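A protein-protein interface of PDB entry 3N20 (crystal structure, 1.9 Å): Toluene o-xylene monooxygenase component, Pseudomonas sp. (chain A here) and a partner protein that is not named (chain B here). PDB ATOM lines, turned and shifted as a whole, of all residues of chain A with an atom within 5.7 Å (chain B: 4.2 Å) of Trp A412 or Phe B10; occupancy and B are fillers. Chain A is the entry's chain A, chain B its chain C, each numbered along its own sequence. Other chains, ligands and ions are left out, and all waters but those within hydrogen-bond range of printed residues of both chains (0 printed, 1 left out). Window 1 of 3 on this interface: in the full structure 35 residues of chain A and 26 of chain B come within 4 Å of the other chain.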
ATOM      1  N   THR A 407     -11.603 -19.881  17.705  1.00  0.00           N
ATOM      2  CA  THR A 407     -10.328 -19.770  18.415  1.00  0.00           C
ATOM      3  C   THR A 407      -9.726 -18.366  18.561  1.00  0.00           C
ATOM      4  O   THR A 407      -9.495 -17.664  17.574  1.00  0.00           O
ATOM      5  CB  THR A 407      -9.265 -20.680  17.772  1.00  0.00           C
ATOM      6  OG1 THR A 407      -9.853 -21.946  17.458  1.00  0.00           O
ATOM      7  CG2 THR A 407      -8.113 -20.902  18.738  1.00  0.00           C
ATOM      8  N   PRO A 408      -9.466 -17.948  19.814  1.00  0.00           N
ATOM      9  CA  PRO A 408      -8.889 -16.655  20.194  1.00  0.00           C
ATOM     10  C   PRO A 408      -7.444 -16.853  20.664  1.00  0.00           C
ATOM     11  O   PRO A 408      -6.830 -17.893  20.410  1.00  0.00           O
ATOM     12  CB  PRO A 408      -9.777 -16.233  21.347  1.00  0.00           C
ATOM     13  CG  PRO A 408      -9.876 -17.541  22.111  1.00  0.00           C
ATOM     14  CD  PRO A 408     -10.064 -18.597  21.000  1.00  0.00           C
ATOM     15  N   GLY A 409      -6.920 -15.849  21.362  1.00  0.00           N
ATOM     16  CA  GLY A 409      -5.571 -15.928  21.895  1.00  0.00           C
ATOM     17  C   GLY A 409      -4.439 -16.115  20.906  1.00  0.00           C
ATOM     18  O   GLY A 409      -4.423 -15.514  19.831  1.00  0.00           O
ATOM     19  N   ASN A 410      -3.489 -16.967  21.276  1.00  0.00           N
ATOM     20  CA  ASN A 410      -2.309 -17.230  20.457  1.00  0.00           C
ATOM     21  C   ASN A 410      -2.512 -17.934  19.123  1.00  0.00           C
ATOM     22  O   ASN A 410      -1.581 -18.026  18.325  1.00  0.00           O
ATOM     23  CB  ASN A 410      -1.279 -17.984  21.290  1.00  0.00           C
ATOM     24  CG  ASN A 410      -0.439 -17.052  22.133  1.00  0.00           C
ATOM     25  OD1 ASN A 410       0.638 -16.616  21.712  1.00  0.00           O
ATOM     26  ND2 ASN A 410      -0.935 -16.714  23.322  1.00  0.00           N
ATOM     27  N   LYS A 411      -3.711 -18.447  18.878  1.00  0.00           N
ATOM     28  CA  LYS A 411      -3.981 -19.098  17.606  1.00  0.00           C
ATOM     29  C   LYS A 411      -5.285 -18.551  17.043  1.00  0.00           C
ATOM     30  O   LYS A 411      -6.146 -19.301  16.593  1.00  0.00           O
ATOM     31  CB  LYS A 411      -4.037 -20.623  17.773  1.00  0.00           C
ATOM     32  CG  LYS A 411      -2.691 -21.224  18.188  1.00  0.00           C
ATOM     33  CD  LYS A 411      -2.413 -22.582  17.543  1.00  0.00           C
ATOM     34  CE  LYS A 411      -2.763 -23.746  18.469  1.00  0.00           C
ATOM     35  NZ  LYS A 411      -2.390 -25.075  17.881  1.00  0.00           N
ATOM     36  N   TRP A 412      -5.404 -17.223  17.072  1.00  0.00           N
ATOM     37  CA  TRP A 412      -6.587 -16.522  16.583  1.00  0.00           C
ATOM     38  C   TRP A 412      -7.000 -17.035  15.217  1.00  0.00           C
ATOM     39  O   TRP A 412      -6.217 -17.003  14.267  1.00  0.00           O
ATOM     40  CB  TRP A 412      -6.321 -15.018  16.508  1.00  0.00           C
ATOM     41  CG  TRP A 412      -7.541 -14.223  16.137  1.00  0.00           C
ATOM     42  CD1 TRP A 412      -8.768 -14.274  16.739  1.00  0.00           C
ATOM     43  CD2 TRP A 412      -7.641 -13.224  15.110  1.00  0.00           C
ATOM     44  NE1 TRP A 412      -9.624 -13.370  16.152  1.00  0.00           N
ATOM     45  CE2 TRP A 412      -8.958 -12.712  15.151  1.00  0.00           C
ATOM     46  CE3 TRP A 412      -6.744 -12.709  14.161  1.00  0.00           C
ATOM     47  CZ2 TRP A 412      -9.402 -11.709  14.281  1.00  0.00           C
ATOM     48  CZ3 TRP A 412      -7.187 -11.709  13.294  1.00  0.00           C
ATOM     49  CH2 TRP A 412      -8.505 -11.221  13.363  1.00  0.00           C
ATOM     50  N   ASN A 413      -8.242 -17.492  15.118  1.00  0.00           N
ATOM     51  CA  ASN A 413      -8.737 -18.049  13.869  1.00  0.00           C
ATOM     52  C   ASN A 413     -10.248 -17.853  13.701  1.00  0.00           C
ATOM     53  O   ASN A 413     -10.957 -18.768  13.280  1.00  0.00           O
ATOM     54  CB  ASN A 413      -8.369 -19.535  13.839  1.00  0.00           C
ATOM     55  CG  ASN A 413      -8.634 -20.180  12.506  1.00  0.00           C
ATOM     56  OD1 ASN A 413      -8.509 -19.543  11.462  1.00  0.00           O
ATOM     57  ND2 ASN A 413      -8.982 -21.465  12.530  1.00  0.00           N
ATOM     58  N   VAL A 414     -10.735 -16.656  14.023  1.00  0.00           N
ATOM     59  CA  VAL A 414     -12.159 -16.346  13.912  1.00  0.00           C
ATOM     60  C   VAL A 414     -12.493 -15.882  12.505  1.00  0.00           C
ATOM     61  O   VAL A 414     -11.899 -14.934  11.995  1.00  0.00           O
ATOM     62  CB  VAL A 414     -12.569 -15.238  14.902  1.00  0.00           C
ATOM     63  CG1 VAL A 414     -14.040 -14.889  14.720  1.00  0.00           C
ATOM     64  CG2 VAL A 414     -12.306 -15.694  16.320  1.00  0.00           C
ATOM     65  N   SER B   8     -17.004  -6.139  13.857  1.00  0.00           N
ATOM     66  CA  SER B   8     -15.630  -6.139  14.327  1.00  0.00           C
ATOM     67  C   SER B   8     -15.091  -7.524  14.672  1.00  0.00           C
ATOM     68  O   SER B   8     -15.615  -8.214  15.543  1.00  0.00           O
ATOM     69  CB  SER B   8     -15.513  -5.219  15.551  1.00  0.00           C
ATOM     70  OG  SER B   8     -14.235  -5.311  16.164  1.00  0.00           O
ATOM     71  N   ASN B   9     -14.045  -7.928  13.964  1.00  0.00           N
ATOM     72  CA  ASN B   9     -13.396  -9.205  14.213  1.00  0.00           C
ATOM     73  C   ASN B   9     -12.036  -8.787  14.775  1.00  0.00           C
ATOM     74  O   ASN B   9     -11.043  -8.677  14.045  1.00  0.00           O
ATOM     75  CB  ASN B   9     -13.247  -9.992  12.905  1.00  0.00           C
ATOM     76  CG  ASN B   9     -12.668 -11.379  13.121  1.00  0.00           C
ATOM     77  OD1 ASN B   9     -12.879 -11.997  14.168  1.00  0.00           O
ATOM     78  ND2 ASN B   9     -11.949 -11.884  12.124  1.00  0.00           N
ATOM     79  N   PHE B  10     -12.019  -8.526  16.079  1.00  0.00           N
ATOM     80  CA  PHE B  10     -10.819  -8.067  16.761  1.00  0.00           C
ATOM     81  C   PHE B  10      -9.788  -9.168  16.960  1.00  0.00           C
ATOM     82  O   PHE B  10     -10.115 -10.263  17.419  1.00  0.00           O
ATOM     83  CB  PHE B  10     -11.188  -7.457  18.111  1.00  0.00           C
ATOM     84  CG  PHE B  10     -10.230  -6.399  18.566  1.00  0.00           C
ATOM     85  CD1 PHE B  10     -10.499  -5.049  18.332  1.00  0.00           C
ATOM     86  CD2 PHE B  10      -9.032  -6.748  19.184  1.00  0.00           C
ATOM     87  CE1 PHE B  10      -9.590  -4.064  18.704  1.00  0.00           C
ATOM     88  CE2 PHE B  10      -8.114  -5.771  19.559  1.00  0.00           C
ATOM     89  CZ  PHE B  10      -8.391  -4.425  19.319  1.00  0.00           C
ATOM     90  N   GLU B  11      -8.534  -8.870  16.626  1.00  0.00           N
ATOM     91  CA  GLU B  11      -7.478  -9.861  16.759  1.00  0.00           C
ATOM     92  C   GLU B  11      -7.321 -10.394  18.180  1.00  0.00           C
ATOM     93  O   GLU B  11      -7.291  -9.631  19.154  1.00  0.00           O
ATOM     94  CB  GLU B  11      -6.140  -9.295  16.268  1.00  0.00           C
ATOM     95  CG  GLU B  11      -4.955 -10.223  16.512  1.00  0.00           C
ATOM     96  CD  GLU B  11      -3.682  -9.751  15.824  1.00  0.00           C
ATOM     97  OE1 GLU B  11      -3.629  -8.575  15.404  1.00  0.00           O
ATOM     98  OE2 GLU B  11      -2.730 -10.555  15.713  1.00  0.00           O
ATOM     99  N   ARG B  12      -7.225 -11.717  18.265  1.00  0.00           N
ATOM    100  CA  ARG B  12      -7.059 -12.447  19.516  1.00  0.00           C
ATOM    101  C   ARG B  12      -8.350 -12.593  20.314  1.00  0.00           C
ATOM    102  O   ARG B  12      -8.370 -13.275  21.343  1.00  0.00           O
ATOM    103  CB  ARG B  12      -5.959 -11.809  20.377  1.00  0.00           C
ATOM    104  CG  ARG B  12      -4.591 -11.776  19.692  1.00  0.00           C
ATOM    105  CD  ARG B  12      -3.505 -11.296  20.644  1.00  0.00           C
ATOM    106  NE  ARG B  12      -3.083 -12.352  21.561  1.00  0.00           N
ATOM    107  CZ  ARG B  12      -2.112 -13.221  21.299  1.00  0.00           C
ATOM    108  NH1 ARG B  12      -1.447 -13.154  20.147  1.00  0.00           N
ATOM    109  NH2 ARG B  12      -1.817 -14.171  22.177  1.00  0.00           N
ATOM    110  N   ASP B  13      -9.428 -11.957  19.854  1.00  0.00           N
ATOM    111  CA  ASP B  13     -10.713 -12.101  20.534  1.00  0.00           C
ATOM    112  C   ASP B  13     -11.306 -13.405  19.993  1.00  0.00           C
ATOM    113  O   ASP B  13     -10.725 -14.024  19.097  1.00  0.00           O
ATOM    114  CB  ASP B  13     -11.653 -10.944  20.211  1.00  0.00           C
ATOM    115  CG  ASP B  13     -12.688 -10.715  21.304  1.00  0.00           C
ATOM    116  OD1 ASP B  13     -13.082 -11.692  21.982  1.00  0.00           O
ATOM    117  OD2 ASP B  13     -13.108  -9.554  21.480  1.00  0.00           O
ATOM    118  N   CYS B  34     -13.862  -0.040  18.026  1.00  0.00           N
ATOM    119  CA  CYS B  34     -13.874  -1.498  18.071  1.00  0.00           C
ATOM    120  C   CYS B  34     -13.131  -2.017  19.311  1.00  0.00           C
ATOM    121  O   CYS B  34     -13.564  -2.982  19.940  1.00  0.00           O
ATOM    122  CB  CYS B  34     -13.221  -2.072  16.807  1.00  0.00           C
ATOM    123  SG  CYS B  34     -14.185  -1.892  15.282  1.00  0.00           S
ATOM    124  N   ALA B  35     -12.013  -1.373  19.653  1.00  0.00           N
ATOM    125  CA  ALA B  35     -11.201  -1.764  20.811  1.00  0.00           C
ATOM    126  C   ALA B  35     -12.004  -1.699  22.106  1.00  0.00           C
ATOM    127  O   ALA B  35     -11.809  -2.502  23.014  1.00  0.00           O
ATOM    128  CB  ALA B  35      -9.974  -0.850  20.922  1.00  0.00           C
ATOM    129  N   SER B  38     -13.357  -4.986  23.047  1.00  0.00           N
ATOM    130  CA  SER B  38     -12.471  -6.145  23.148  1.00  0.00           C
ATOM    131  C   SER B  38     -11.283  -5.955  24.091  1.00  0.00           C
ATOM    132  O   SER B  38     -11.003  -6.828  24.916  1.00  0.00           O
ATOM    133  CB  SER B  38     -11.968  -6.541  21.760  1.00  0.00           C
ATOM    134  OG  SER B  38     -13.045  -6.947  20.933  1.00  0.00           O
ATOM    135  N   ILE B  39     -10.584  -4.829  23.965  1.00  0.00           N
ATOM    136  CA  ILE B  39      -9.426  -4.548  24.814  1.00  0.00           C
ATOM    137  C   ILE B  39      -9.885  -4.352  26.256  1.00  0.00           C
ATOM    138  O   ILE B  39     -10.862  -3.641  26.519  1.00  0.00           O
ATOM    139  CB  ILE B  39      -8.662  -3.279  24.332  1.00  0.00           C
ATOM    140  CG1 ILE B  39      -8.129  -3.494  22.909  1.00  0.00           C
ATOM    141  CG2 ILE B  39      -7.506  -2.958  25.285  1.00  0.00           C
ATOM    142  CD1 ILE B  39      -7.098  -4.612  22.784  1.00  0.00           C
ATOM    143  N   LEU B  51      -3.189  -0.350  15.978  1.00  0.00           N
ATOM    144  CA  LEU B  51      -4.372  -1.038  15.475  1.00  0.00           C
ATOM    145  C   LEU B  51      -4.697  -0.608  14.051  1.00  0.00           C
ATOM    146  O   LEU B  51      -4.852   0.584  13.769  1.00  0.00           O
ATOM    147  CB  LEU B  51      -5.578  -0.755  16.376  1.00  0.00           C
ATOM    148  CG  LEU B  51      -5.536  -1.380  17.767  1.00  0.00           C
ATOM    149  CD1 LEU B  51      -6.779  -0.989  18.549  1.00  0.00           C
ATOM    150  CD2 LEU B  51      -5.444  -2.896  17.625  1.00  0.00           C
ATOM    151  N   ASP B  80     -11.419  -6.821  10.081  1.00  0.00           N
ATOM    152  CA  ASP B  80     -10.446  -7.351  11.027  1.00  0.00           C
ATOM    153  C   ASP B  80      -9.757  -6.136  11.647  1.00  0.00           C
ATOM    154  O   ASP B  80      -9.416  -5.186  10.945  1.00  0.00           O
ATOM    155  CB  ASP B  80      -9.377  -8.205  10.335  1.00  0.00           C
ATOM    156  CG  ASP B  80      -9.943  -9.446   9.678  1.00  0.00           C
ATOM    157  OD1 ASP B  80     -10.921 -10.015  10.209  1.00  0.00           O
ATOM    158  OD2 ASP B  80      -9.391  -9.862   8.636  1.00  0.00           O
ATOM    159  N   ILE B  81      -9.583  -6.154  12.961  1.00  0.00           N
ATOM    160  CA  ILE B  81      -8.899  -5.071  13.651  1.00  0.00           C
ATOM    161  C   ILE B  81      -7.648  -5.775  14.155  1.00  0.00           C
ATOM    162  O   ILE B  81      -7.704  -6.563  15.103  1.00  0.00           O
ATOM    163  CB  ILE B  81      -9.730  -4.529  14.832  1.00  0.00           C
ATOM    164  CG1 ILE B  81     -11.170  -4.251  14.378  1.00  0.00           C
ATOM    165  CG2 ILE B  81      -9.096  -3.242  15.360  1.00  0.00           C
ATOM    166  CD1 ILE B  81     -11.305  -3.181  13.299  1.00  0.00           C
ATOM    167  N   PHE B  83      -3.229  -5.931  15.106  1.00  0.00           N
ATOM    168  CA  PHE B  83      -2.076  -5.280  15.733  1.00  0.00           C
ATOM    169  C   PHE B  83      -0.911  -5.270  14.739  1.00  0.00           C
ATOM    170  O   PHE B  83      -0.516  -6.326  14.240  1.00  0.00           O
ATOM    171  CB  PHE B  83      -1.649  -6.061  16.980  1.00  0.00           C
ATOM    172  CG  PHE B  83      -2.659  -6.038  18.094  1.00  0.00           C
ATOM    173  CD1 PHE B  83      -2.758  -4.933  18.931  1.00  0.00           C
ATOM    174  CD2 PHE B  83      -3.507  -7.120  18.309  1.00  0.00           C
ATOM    175  CE1 PHE B  83      -3.687  -4.903  19.972  1.00  0.00           C
ATOM    176  CE2 PHE B  83      -4.440  -7.100  19.346  1.00  0.00           C
ATOM    177  CZ  PHE B  83      -4.529  -5.988  20.180  1.00  0.00           C
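Thr A407 touches none of the printed residues of chain B. Trp A412 touches just these residues of chain B: Asn B9, Phe B10, Glu B11, Arg B12 and Asp B13. Of the printed residues of chain B, Val A414 touches Asn B9 (3.1 Å) and Asp B13 (3.6 Å). Printed residues of chain A within 4 Å of Asn B9: Trp A412 and Val A414. Of chain A, only Trp A412 comes within 4 Å of Phe B10. The nearest printed residue of chain A that does not touch Glu B11 is Gly A409 (6.1 Å).
Arg B12 touches Pro A408. O of Asp B13 touches CB of Pro A408, at 3.3 Å. Asn B9 touches Trp A412. CE2 of Trp A412 touches CA of Glu B11, 3.6 Å away. Arg B12 touches Trp A412 (N to CG, 3.3 Å). Val A414 touches Asp B13 (CG2 to O, 3.6 Å).
O of Arg B12 is in hydrogen-bond range of N of Gly A409, at 3.0 Å. ND2 of Asn A410 sits close to NH2 of Arg B12. The backbone carbonyl oxygen (O) of Phe B10 lies within hydrogen-bond range of the indole nitrogen (NE1) of Trp A412, at 3.4 Å. NE1 of Trp A412 lies close to O of Asp B13, at 3.2 Å. ND2 of Asn B9 sits at hydrogen-bond distance from O of Val A414 (3.1 Å).
OD1 of Asp B80 sits at hydrogen-bond distance from ND2 of Asn B9. The backbone NH (N) of Ile B81 lies within hydrogen-bond range of the backbone carbonyl oxygen (O) of Asn B9, 3.1 Å away. The backbone NH (N) of Glu B11 lies within hydrogen-bond range of the backbone carbonyl oxygen (O) of Ile B81 (2.9 Å). The side-chain carboxylate (OE1) of Glu B11 lies within hydrogen-bond range of the backbone NH (N) of Phe B83 (2.7 Å). The side-chain carboxylate (OD2) of Asp B13 lies within hydrogen-bond range of the side-chain hydroxyl (OG) of Ser B38.
Of the 8 printed residues of chain A, 5 touch a printed residue of chain B. Hydrophobic or aromatic side chains of chain A that line the printed part of chain B: Pro A408, Trp A412 and Val A414. Of the 14 printed residues of chain B, 5 touch a printed residue of chain A. Along chain B the printed residues that touch a printed residue of chain A span positions 9 to 13. Among the printed residues, 11 pairs touch across the chains. Among the printed residues, no Asp or Glu carboxylate lies within 4 Å of a Lys or Arg side-chain nitrogen of the other chain.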
